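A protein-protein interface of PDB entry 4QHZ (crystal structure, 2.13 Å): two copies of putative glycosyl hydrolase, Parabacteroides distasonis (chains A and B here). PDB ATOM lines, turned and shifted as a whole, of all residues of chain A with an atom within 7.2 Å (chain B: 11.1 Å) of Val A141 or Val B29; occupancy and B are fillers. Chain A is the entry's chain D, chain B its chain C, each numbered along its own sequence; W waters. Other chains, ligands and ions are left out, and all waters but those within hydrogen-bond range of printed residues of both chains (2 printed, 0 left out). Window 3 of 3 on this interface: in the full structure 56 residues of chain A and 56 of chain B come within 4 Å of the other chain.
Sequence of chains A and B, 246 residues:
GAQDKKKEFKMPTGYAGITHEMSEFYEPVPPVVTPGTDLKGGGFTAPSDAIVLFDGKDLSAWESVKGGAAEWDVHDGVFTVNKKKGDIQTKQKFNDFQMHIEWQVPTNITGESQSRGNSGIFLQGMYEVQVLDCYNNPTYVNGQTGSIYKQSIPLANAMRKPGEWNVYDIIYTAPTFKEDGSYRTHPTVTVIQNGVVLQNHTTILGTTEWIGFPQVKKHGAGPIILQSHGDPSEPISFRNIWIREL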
ATOM      1  N   GLN A 114      22.812 -14.444  26.991  1.00  0.00           N
ATOM      2  CA  GLN A 114      23.602 -13.212  26.937  1.00  0.00           C
ATOM      3  C   GLN A 114      23.432 -12.307  28.164  1.00  0.00           C
ATOM      4  O   GLN A 114      24.147 -11.313  28.289  1.00  0.00           O
ATOM      5  CB  GLN A 114      23.260 -12.409  25.676  1.00  0.00           C
ATOM      6  CG  GLN A 114      23.573 -13.128  24.374  1.00  0.00           C
ATOM      7  CD  GLN A 114      25.066 -13.231  24.097  1.00  0.00           C
ATOM      8  OE1 GLN A 114      25.778 -12.225  24.090  1.00  0.00           O
ATOM      9  NE2 GLN A 114      25.548 -14.453  23.858  1.00  0.00           N
ATOM     10  N   PRO A 138      24.059 -22.211  28.202  1.00  0.00           N
ATOM     11  CA  PRO A 138      24.092 -22.167  26.740  1.00  0.00           C
ATOM     12  C   PRO A 138      23.645 -20.809  26.196  1.00  0.00           C
ATOM     13  O   PRO A 138      22.881 -20.084  26.847  1.00  0.00           O
ATOM     14  CB  PRO A 138      23.113 -23.274  26.321  1.00  0.00           C
ATOM     15  CG  PRO A 138      22.250 -23.523  27.506  1.00  0.00           C
ATOM     16  CD  PRO A 138      23.041 -23.149  28.721  1.00  0.00           C
ATOM     17  N   THR A 139      24.150 -20.465  25.021  1.00  0.00           N
ATOM     18  CA  THR A 139      23.760 -19.255  24.314  1.00  0.00           C
ATOM     19  C   THR A 139      24.080 -19.466  22.845  1.00  0.00           C
ATOM     20  O   THR A 139      24.506 -20.562  22.456  1.00  0.00           O
ATOM     21  CB  THR A 139      24.486 -18.009  24.876  1.00  0.00           C
ATOM     22  OG1 THR A 139      23.932 -16.815  24.300  1.00  0.00           O
ATOM     23  CG2 THR A 139      25.995 -18.064  24.595  1.00  0.00           C
ATOM     24  N   TYR A 140      23.887 -18.445  22.017  1.00  0.00           N
ATOM     25  CA  TYR A 140      24.257 -18.589  20.604  1.00  0.00           C
ATOM     26  C   TYR A 140      25.773 -18.638  20.505  1.00  0.00           C
ATOM     27  O   TYR A 140      26.477 -17.839  21.125  1.00  0.00           O
ATOM     28  CB  TYR A 140      23.642 -17.511  19.690  1.00  0.00           C
ATOM     29  CG  TYR A 140      23.675 -16.071  20.152  1.00  0.00           C
ATOM     30  CD1 TYR A 140      22.611 -15.529  20.872  1.00  0.00           C
ATOM     31  CD2 TYR A 140      24.730 -15.229  19.805  1.00  0.00           C
ATOM     32  CE1 TYR A 140      22.613 -14.200  21.271  1.00  0.00           C
ATOM     33  CE2 TYR A 140      24.744 -13.901  20.200  1.00  0.00           C
ATOM     34  CZ  TYR A 140      23.686 -13.390  20.933  1.00  0.00           C
ATOM     35  OH  TYR A 140      23.680 -12.073  21.316  1.00  0.00           O
ATOM     36  N   VAL A 141      26.265 -19.621  19.751  1.00  0.00           N
ATOM     37  CA  VAL A 141      27.675 -20.023  19.831  1.00  0.00           C
ATOM     38  C   VAL A 141      28.614 -18.979  19.238  1.00  0.00           C
ATOM     39  O   VAL A 141      29.751 -18.842  19.692  1.00  0.00           O
ATOM     40  CB  VAL A 141      27.942 -21.405  19.170  1.00  0.00           C
ATOM     41  CG1 VAL A 141      27.182 -22.495  19.905  1.00  0.00           C
ATOM     42  CG2 VAL A 141      27.591 -21.406  17.676  1.00  0.00           C
ATOM     43  N   ASN A 142      28.139 -18.239  18.239  1.00  0.00           N
ATOM     44  CA  ASN A 142      28.942 -17.161  17.655  1.00  0.00           C
ATOM     45  C   ASN A 142      28.983 -15.912  18.551  1.00  0.00           C
ATOM     46  O   ASN A 142      29.645 -14.943  18.213  1.00  0.00           O
ATOM     47  CB  ASN A 142      28.461 -16.809  16.235  1.00  0.00           C
ATOM     48  CG  ASN A 142      27.028 -16.304  16.197  1.00  0.00           C
ATOM     49  OD1 ASN A 142      26.163 -16.775  16.940  1.00  0.00           O
ATOM     50  ND2 ASN A 142      26.764 -15.351  15.313  1.00  0.00           N
ATOM     51  N   GLY A 143      28.272 -15.942  19.678  1.00  0.00           N
ATOM     52  CA  GLY A 143      28.327 -14.855  20.655  1.00  0.00           C
ATOM     53  C   GLY A 143      28.655 -15.304  22.070  1.00  0.00           C
ATOM     54  O   GLY A 143      28.424 -14.562  23.027  1.00  0.00           O
ATOM     55  N   GLN A 144      29.190 -16.513  22.221  1.00  0.00           N
ATOM     56  CA  GLN A 144      29.533 -17.010  23.553  1.00  0.00           C
ATOM     57  C   GLN A 144      30.939 -16.543  23.951  1.00  0.00           C
ATOM     58  O   GLN A 144      31.605 -15.831  23.198  1.00  0.00           O
ATOM     59  CB  GLN A 144      29.371 -18.538  23.628  1.00  0.00           C
ATOM     60  CG  GLN A 144      30.490 -19.380  23.045  1.00  0.00           C
ATOM     61  CD  GLN A 144      30.172 -20.862  23.140  1.00  0.00           C
ATOM     62  OE1 GLN A 144      29.164 -21.318  22.609  1.00  0.00           O
ATOM     63  NE2 GLN A 144      31.020 -21.617  23.827  1.00  0.00           N
ATOM     64  N   THR A 145      31.375 -16.949  25.138  1.00  0.00           N
ATOM     65  CA  THR A 145      32.644 -16.508  25.704  1.00  0.00           C
ATOM     66  C   THR A 145      33.823 -16.735  24.759  1.00  0.00           C
ATOM     67  O   THR A 145      33.996 -17.823  24.223  1.00  0.00           O
ATOM     68  CB  THR A 145      32.935 -17.250  27.019  1.00  0.00           C
ATOM     69  OG1 THR A 145      31.780 -17.172  27.868  1.00  0.00           O
ATOM     70  CG2 THR A 145      34.141 -16.645  27.721  1.00  0.00           C
ATOM     71  N   GLY A 146      34.626 -15.697  24.552  1.00  0.00           N
ATOM     72  CA  GLY A 146      35.807 -15.800  23.704  1.00  0.00           C
ATOM     73  C   GLY A 146      35.541 -15.697  22.217  1.00  0.00           C
ATOM     74  O   GLY A 146      36.470 -15.784  21.414  1.00  0.00           O
ATOM     75  N   SER A 147      34.279 -15.517  21.833  1.00  0.00           N
ATOM     76  CA  SER A 147      33.947 -15.267  20.445  1.00  0.00           C
ATOM     77  C   SER A 147      34.460 -13.900  20.063  1.00  0.00           C
ATOM     78  O   SER A 147      34.627 -13.040  20.931  1.00  0.00           O
ATOM     79  CB  SER A 147      32.432 -15.342  20.210  1.00  0.00           C
ATOM     80  OG  SER A 147      31.726 -14.334  20.919  1.00  0.00           O
ATOM     81  N   LYS A 150      29.740 -12.452  17.334  1.00  0.00           N
ATOM     82  CA  LYS A 150      28.876 -12.730  16.173  1.00  0.00           C
ATOM     83  C   LYS A 150      29.608 -12.872  14.831  1.00  0.00           C
ATOM     84  O   LYS A 150      28.996 -12.766  13.768  1.00  0.00           O
ATOM     85  CB  LYS A 150      27.753 -11.675  16.067  1.00  0.00           C
ATOM     86  CG  LYS A 150      26.635 -11.882  17.079  1.00  0.00           C
ATOM     87  CD  LYS A 150      25.393 -11.083  16.728  1.00  0.00           C
ATOM     88  CE  LYS A 150      24.222 -11.470  17.609  1.00  0.00           C
ATOM     89  NZ  LYS A 150      22.939 -10.913  17.099  1.00  0.00           N
ATOM     90  N   SER A 152      33.109 -14.989  14.771  1.00  0.00           N
ATOM     91  CA  SER A 152      33.950 -16.172  14.874  1.00  0.00           C
ATOM     92  C   SER A 152      33.674 -16.951  16.152  1.00  0.00           C
ATOM     93  O   SER A 152      33.881 -16.451  17.256  1.00  0.00           O
ATOM     94  CB  SER A 152      35.415 -15.757  14.837  1.00  0.00           C
ATOM     95  OG  SER A 152      35.704 -15.074  13.634  1.00  0.00           O
ATOM     96  N   ILE A 153      33.193 -18.179  15.981  1.00  0.00           N
ATOM     97  CA  ILE A 153      32.877 -19.072  17.072  1.00  0.00           C
ATOM     98  C   ILE A 153      34.181 -19.511  17.725  1.00  0.00           C
ATOM     99  O   ILE A 153      35.132 -19.868  17.025  1.00  0.00           O
ATOM    100  CB  ILE A 153      32.104 -20.305  16.558  1.00  0.00           C
ATOM    101  CG1 ILE A 153      30.785 -19.888  15.894  1.00  0.00           C
ATOM    102  CG2 ILE A 153      31.811 -21.278  17.690  1.00  0.00           C
ATOM    103  CD1 ILE A 153      30.193 -20.941  14.989  1.00  0.00           C
ATOM    104  N   PRO A 154      34.241 -19.493  19.067  1.00  0.00           N
ATOM    105  CA  PRO A 154      35.471 -19.920  19.721  1.00  0.00           C
ATOM    106  C   PRO A 154      35.706 -21.418  19.568  1.00  0.00           C
ATOM    107  O   PRO A 154      34.748 -22.193  19.435  1.00  0.00           O
ATOM    108  CB  PRO A 154      35.227 -19.568  21.188  1.00  0.00           C
ATOM    109  CG  PRO A 154      33.749 -19.624  21.342  1.00  0.00           C
ATOM    110  CD  PRO A 154      33.210 -19.105  20.041  1.00  0.00           C
ATOM    111  N   LEU A 155      36.973 -21.818  19.597  1.00  0.00           N
ATOM    112  CA  LEU A 155      37.351 -23.215  19.386  1.00  0.00           C
ATOM    113  C   LEU A 155      36.952 -24.128  20.546  1.00  0.00           C
ATOM    114  O   LEU A 155      36.892 -25.344  20.390  1.00  0.00           O
ATOM    115  CB  LEU A 155      38.859 -23.318  19.143  1.00  0.00           C
ATOM    116  CG  LEU A 155      39.357 -22.616  17.869  1.00  0.00           C
ATOM    117  CD1 LEU A 155      40.874 -22.521  17.858  1.00  0.00           C
ATOM    118  CD2 LEU A 155      38.846 -23.337  16.629  1.00  0.00           C
ATOM    119  N   ALA A 156      36.681 -23.552  21.707  1.00  0.00           N
ATOM    120  CA  ALA A 156      36.268 -24.342  22.856  1.00  0.00           C
ATOM    121  C   ALA A 156      35.513 -23.493  23.863  1.00  0.00           C
ATOM    122  O   ALA A 156      35.488 -22.268  23.769  1.00  0.00           O
ATOM    123  CB  ALA A 156      37.485 -24.973  23.515  1.00  0.00           C
ATOM    124  N   ASN A 157      34.884 -24.177  24.808  1.00  0.00           N
ATOM    125  CA  ASN A 157      34.379 -23.574  26.014  1.00  0.00           C
ATOM    126  C   ASN A 157      35.326 -23.976  27.143  1.00  0.00           C
ATOM    127  O   ASN A 157      35.323 -25.125  27.571  1.00  0.00           O
ATOM    128  CB  ASN A 157      32.952 -24.035  26.277  1.00  0.00           C
ATOM    129  CG  ASN A 157      32.350 -23.420  27.527  1.00  0.00           C
ATOM    130  OD1 ASN A 157      33.056 -23.097  28.479  1.00  0.00           O
ATOM    131  ND2 ASN A 157      31.023 -23.283  27.543  1.00  0.00           N
ATOM    132  N   HIS B  20      18.296  -8.956  15.038  1.00  0.00           N
ATOM    133  CA  HIS B  20      19.441  -9.509  15.762  1.00  0.00           C
ATOM    134  C   HIS B  20      19.465 -11.050  15.724  1.00  0.00           C
ATOM    135  O   HIS B  20      20.542 -11.646  15.703  1.00  0.00           O
ATOM    136  CB  HIS B  20      19.505  -8.974  17.206  1.00  0.00           C
ATOM    137  CG  HIS B  20      18.429  -9.488  18.109  1.00  0.00           C
ATOM    138  ND1 HIS B  20      18.595 -10.600  18.902  1.00  0.00           N
ATOM    139  CD2 HIS B  20      17.187  -9.020  18.372  1.00  0.00           C
ATOM    140  CE1 HIS B  20      17.492 -10.807  19.602  1.00  0.00           C
ATOM    141  NE2 HIS B  20      16.622  -9.863  19.297  1.00  0.00           N
ATOM    142  N   GLU B  21      18.288 -11.677  15.685  1.00  0.00           N
ATOM    143  CA  GLU B  21      18.175 -13.136  15.644  1.00  0.00           C
ATOM    144  C   GLU B  21      18.813 -13.748  14.398  1.00  0.00           C
ATOM    145  O   GLU B  21      19.277 -14.886  14.436  1.00  0.00           O
ATOM    146  CB  GLU B  21      16.706 -13.589  15.706  1.00  0.00           C
ATOM    147  CG  GLU B  21      16.025 -13.360  17.052  1.00  0.00           C
ATOM    148  CD  GLU B  21      15.211 -12.078  17.103  1.00  0.00           C
ATOM    149  OE1 GLU B  21      15.485 -11.153  16.307  1.00  0.00           O
ATOM    150  OE2 GLU B  21      14.294 -11.995  17.945  1.00  0.00           O
ATOM    151  N   SER B  23      21.507 -13.194  13.023  1.00  0.00           N
ATOM    152  CA  SER B  23      22.944 -13.420  13.166  1.00  0.00           C
ATOM    153  C   SER B  23      23.269 -14.165  14.464  1.00  0.00           C
ATOM    154  O   SER B  23      24.348 -14.002  15.017  1.00  0.00           O
ATOM    155  CB  SER B  23      23.712 -12.090  13.089  1.00  0.00           C
ATOM    156  OG  SER B  23      23.268 -11.169  14.069  1.00  0.00           O
ATOM    157  N   GLU B  24      22.331 -14.988  14.934  1.00  0.00           N
ATOM    158  CA  GLU B  24      22.511 -15.779  16.156  1.00  0.00           C
ATOM    159  C   GLU B  24      22.385 -17.271  15.840  1.00  0.00           C
ATOM    160  O   GLU B  24      21.304 -17.759  15.540  1.00  0.00           O
ATOM    161  CB  GLU B  24      21.498 -15.342  17.222  1.00  0.00           C
ATOM    162  CG  GLU B  24      21.823 -13.958  17.773  1.00  0.00           C
ATOM    163  CD  GLU B  24      20.703 -13.286  18.541  1.00  0.00           C
ATOM    164  OE1 GLU B  24      19.670 -13.924  18.847  1.00  0.00           O
ATOM    165  OE2 GLU B  24      20.871 -12.085  18.845  1.00  0.00           O
ATOM    166  N   PHE B  25      23.512 -17.977  15.893  1.00  0.00           N
ATOM    167  CA  PHE B  25      23.595 -19.382  15.492  1.00  0.00           C
ATOM    168  C   PHE B  25      23.882 -20.271  16.690  1.00  0.00           C
ATOM    169  O   PHE B  25      24.555 -19.854  17.629  1.00  0.00           O
ATOM    170  CB  PHE B  25      24.677 -19.541  14.428  1.00  0.00           C
ATOM    171  CG  PHE B  25      24.519 -18.589  13.280  1.00  0.00           C
ATOM    172  CD1 PHE B  25      23.494 -18.755  12.376  1.00  0.00           C
ATOM    173  CD2 PHE B  25      25.386 -17.512  13.118  1.00  0.00           C
ATOM    174  CE1 PHE B  25      23.331 -17.877  11.320  1.00  0.00           C
ATOM    175  CE2 PHE B  25      25.222 -16.623  12.066  1.00  0.00           C
ATOM    176  CZ  PHE B  25      24.189 -16.804  11.169  1.00  0.00           C
ATOM    177  N   TYR B  26      23.351 -21.492  16.662  1.00  0.00           N
ATOM    178  CA  TYR B  26      23.421 -22.402  17.816  1.00  0.00           C
ATOM    179  C   TYR B  26      24.235 -23.669  17.530  1.00  0.00           C
ATOM    180  O   TYR B  26      24.275 -24.581  18.349  1.00  0.00           O
ATOM    181  CB  TYR B  26      21.997 -22.715  18.291  1.00  0.00           C
ATOM    182  CG  TYR B  26      21.337 -21.466  18.817  1.00  0.00           C
ATOM    183  CD1 TYR B  26      20.691 -20.578  17.958  1.00  0.00           C
ATOM    184  CD2 TYR B  26      21.431 -21.125  20.160  1.00  0.00           C
ATOM    185  CE1 TYR B  26      20.118 -19.409  18.432  1.00  0.00           C
ATOM    186  CE2 TYR B  26      20.862 -19.958  20.646  1.00  0.00           C
ATOM    187  CZ  TYR B  26      20.211 -19.105  19.781  1.00  0.00           C
ATOM    188  OH  TYR B  26      19.656 -17.951  20.270  1.00  0.00           O
ATOM    189  N   GLU B  27      24.898 -23.688  16.378  1.00  0.00           N
ATOM    190  CA  GLU B  27      25.804 -24.748  15.978  1.00  0.00           C
ATOM    191  C   GLU B  27      26.850 -24.158  15.038  1.00  0.00           C
ATOM    192  O   GLU B  27      26.585 -23.167  14.388  1.00  0.00           O
ATOM    193  CB  GLU B  27      25.085 -25.876  15.250  1.00  0.00           C
ATOM    194  CG  GLU B  27      24.384 -26.925  16.101  1.00  0.00           C
ATOM    195  CD  GLU B  27      23.322 -27.681  15.318  1.00  0.00           C
ATOM    196  OE1 GLU B  27      22.338 -27.049  14.886  1.00  0.00           O
ATOM    197  OE2 GLU B  27      23.461 -28.910  15.141  1.00  0.00           O
ATOM    198  N   PRO B  28      28.046 -24.758  14.957  1.00  0.00           N
ATOM    199  CA  PRO B  28      28.525 -25.890  15.745  1.00  0.00           C
ATOM    200  C   PRO B  28      28.848 -25.479  17.183  1.00  0.00           C
ATOM    201  O   PRO B  28      29.383 -24.392  17.413  1.00  0.00           O
ATOM    202  CB  PRO B  28      29.796 -26.318  15.007  1.00  0.00           C
ATOM    203  CG  PRO B  28      30.275 -25.084  14.325  1.00  0.00           C
ATOM    204  CD  PRO B  28      29.035 -24.328  13.951  1.00  0.00           C
ATOM    205  N   VAL B  29      28.521 -26.356  18.131  1.00  0.00           N
ATOM    206  CA  VAL B  29      28.744 -26.102  19.547  1.00  0.00           C
ATOM    207  C   VAL B  29      30.201 -26.365  19.897  1.00  0.00           C
ATOM    208  O   VAL B  29      30.690 -27.464  19.675  1.00  0.00           O
ATOM    209  CB  VAL B  29      27.852 -26.997  20.428  1.00  0.00           C
ATOM    210  CG1 VAL B  29      28.063 -26.686  21.906  1.00  0.00           C
ATOM    211  CG2 VAL B  29      26.386 -26.817  20.057  1.00  0.00           C
ATOM    212  N   PRO B  30      30.908 -25.359  20.444  1.00  0.00           N
ATOM    213  CA  PRO B  30      32.291 -25.610  20.860  1.00  0.00           C
ATOM    214  C   PRO B  30      32.367 -26.630  21.998  1.00  0.00           C
ATOM    215  O   PRO B  30      31.532 -26.587  22.905  1.00  0.00           O
ATOM    216  CB  PRO B  30      32.772 -24.242  21.358  1.00  0.00           C
ATOM    217  CG  PRO B  30      31.851 -23.255  20.735  1.00  0.00           C
ATOM    218  CD  PRO B  30      30.531 -23.946  20.624  1.00  0.00           C
ATOM    219  N   PRO B  31      33.357 -27.543  21.951  1.00  0.00           N
ATOM    220  CA  PRO B  31      33.465 -28.551  23.009  1.00  0.00           C
ATOM    221  C   PRO B  31      33.795 -27.928  24.359  1.00  0.00           C
ATOM    222  O   PRO B  31      34.549 -26.955  24.423  1.00  0.00           O
ATOM    223  CB  PRO B  31      34.611 -29.458  22.535  1.00  0.00           C
ATOM    224  CG  PRO B  31      35.373 -28.647  21.549  1.00  0.00           C
ATOM    225  CD  PRO B  31      34.377 -27.728  20.905  1.00  0.00           C
ATOM    226  N   VAL B  32      33.214 -28.485  25.415  1.00  0.00           N
ATOM    227  CA  VAL B  32      33.500 -28.066  26.776  1.00  0.00           C
ATOM    228  C   VAL B  32      34.806 -28.703  27.234  1.00  0.00           C
ATOM    229  O   VAL B  32      34.952 -29.923  27.208  1.00  0.00           O
ATOM    230  CB  VAL B  32      32.371 -28.459  27.751  1.00  0.00           C
ATOM    231  CG1 VAL B  32      32.719 -28.039  29.173  1.00  0.00           C
ATOM    232  CG2 VAL B  32      31.058 -27.831  27.315  1.00  0.00           C
ATOM    233  N   VAL B  33      35.743 -27.860  27.650  1.00  0.00           N
ATOM    234  CA  VAL B  33      37.036 -28.287  28.162  1.00  0.00           C
ATOM    235  C   VAL B  33      37.204 -27.759  29.567  1.00  0.00           C
ATOM    236  O   VAL B  33      36.943 -26.582  29.821  1.00  0.00           O
ATOM    237  CB  VAL B  33      38.174 -27.741  27.294  1.00  0.00           C
ATOM    238  CG1 VAL B  33      39.523 -28.029  27.928  1.00  0.00           C
ATOM    239  CG2 VAL B  33      38.094 -28.332  25.893  1.00  0.00           C
ATOM    240  N   ASP B  49      41.132 -32.072  27.709  1.00  0.00           N
ATOM    241  CA  ASP B  49      41.264 -32.702  26.393  1.00  0.00           C
ATOM    242  C   ASP B  49      42.716 -32.785  25.897  1.00  0.00           C
ATOM    243  O   ASP B  49      42.964 -33.192  24.765  1.00  0.00           O
ATOM    244  CB  ASP B  49      40.408 -31.956  25.362  1.00  0.00           C
ATOM    245  CG  ASP B  49      40.948 -30.570  25.024  1.00  0.00           C
ATOM    246  OD1 ASP B  49      41.735 -30.005  25.813  1.00  0.00           O
ATOM    247  OD2 ASP B  49      40.568 -30.036  23.967  1.00  0.00           O
HETATM  248  O   HOH W   1      21.168 -11.162  21.694  1.00  0.00           O
HETATM  249  O   HOH W   2      30.260 -24.438  24.320  1.00  0.00           O
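The backbone carbonyl oxygen of His B20 sits at hydrogen-bond distance from the side-chain hydroxyl of Ser B23, at 3.2 Å.
The backbone carbonyl oxygen (O) of Asn A142 lies close to the side-chain hydroxyl (OG) of Ser A147 (3.5 Å).
The side-chain amide oxygen of Gln A114 lies close to the side-chain hydroxyl of Tyr A140 (3.5 Å).
The side-chain hydroxyl (OG1) of Thr A139 sits at hydrogen-bond distance from the side-chain amide nitrogen (NE2) of Gln A114 (2.9 Å).
O of Asn A142 sits at hydrogen-bond distance from N of Lys A150 (2.6 Å).
OE2 of Glu B21 sits close to NE2 of His B20, 3.4 Å away.
Thr A139 touches Tyr B26 (O to CD2, 3.9 Å).
Val A141 touches Tyr B26.
Glu B27 touches Val A141.
Pro B30 touches Val A141.
Gln A144 touches Pro B30.
Ile A153 touches Pro B28 (CD1 to CD, 3.7 Å).
CG2 of Ile A153 touches CG of Pro B30, 3.6 Å away.
O of Pro A154 touches CG of Pro B30, at 3.3 Å.
CB of Pro B30 touches C of Ala A156, 3.8 Å away.
CA of Ala A156 touches O of Pro B31 (3.5 Å).
The backbone carbonyl oxygen (O) of Ser B23 sits at hydrogen-bond distance from the side-chain amide nitrogen (ND2) of Asn A142 (2.8 Å).
NZ of Lys A150 lies within salt-bridge range of OE2 of Glu B24, at 2.9 Å.
O of His B20 sits at hydrogen-bond distance from NZ of Lys A150 (2.9 Å).
N of Phe B25 lies within hydrogen-bond range of OD1 of Asn A142, at 3.1 Å.
N of Asn A157 lies within hydrogen-bond range of O of Pro B31 (2.8 Å).
The backbone NH (N) of Val B33 sits at hydrogen-bond distance from the backbone carbonyl oxygen (O) of Asn A157, 2.8 Å away.
OG of Ser B23 is in hydrogen-bond range of NZ of Lys A150.
The backbone carbonyl oxygen (O) of Phe B25 lies within hydrogen-bond range of the backbone NH (N) of Val A141.
No position is printed for both chains.
Printed residues of chain B that touch a printed residue of chain A: His B20, Ser B23, Glu B24, Phe B25, Tyr B26, Glu B27, Pro B28, Val B29, Pro B30, Pro B31, Val B32 and Val B33.
Hydrophobic or aromatic side chains of chain B that line the printed part of chain A: His B20, Phe B25, Tyr B26, Pro B28, Pro B30, Pro B31 and Val B33.
Of the 18 printed residues of chain A, 11 touch a printed residue of chain B.
Along chain A the printed residues that touch a printed residue of chain B span positions 139 to 157.
Of chain B, only Phe B25, Tyr B26, Glu B27, Pro B28, Val B29 and Pro B30 come within 4 Å of Val A141.
Val B29 touches just one residue of chain A: Val A141.
Of chain B, only Pro B28 and Pro B30 come within 4 Å of Ile A153.
Printed residues of chain B within 4 Å of Pro A154: Pro B30.
Printed residues of chain A within 4 Å of Tyr B26: Thr A139 (3.9 Å), Tyr A140 (3.6 Å) and Val A141 (3.9 Å).
Of the printed residues of chain A, Pro B31 touches Leu A155, Ala A156 and Asn A157.
Of the printed residues of chain A, His B20 touches Lys A150 (2.9 Å).
Ser A152 touches none of the printed residues of chain B.
The nearest residue of chain B that does not touch Val A141 is Glu B24 (6.0 Å).
The nearest residue of chain A that does not touch Val B29 is Gln A144 (5.5 Å).
The nearest printed residue of chain B that does not touch Tyr A140 is Ser B23 (5.0 Å).
Water W1 lies within hydrogen-bond range of OH of Tyr A140 and OE2 of Glu B24.
Water W2 lies within hydrogen-bond range of the backbone carbonyl oxygen of Pro B30 (2.9 Å) and the side-chain amide nitrogen of Gln A144 (3.0 Å).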
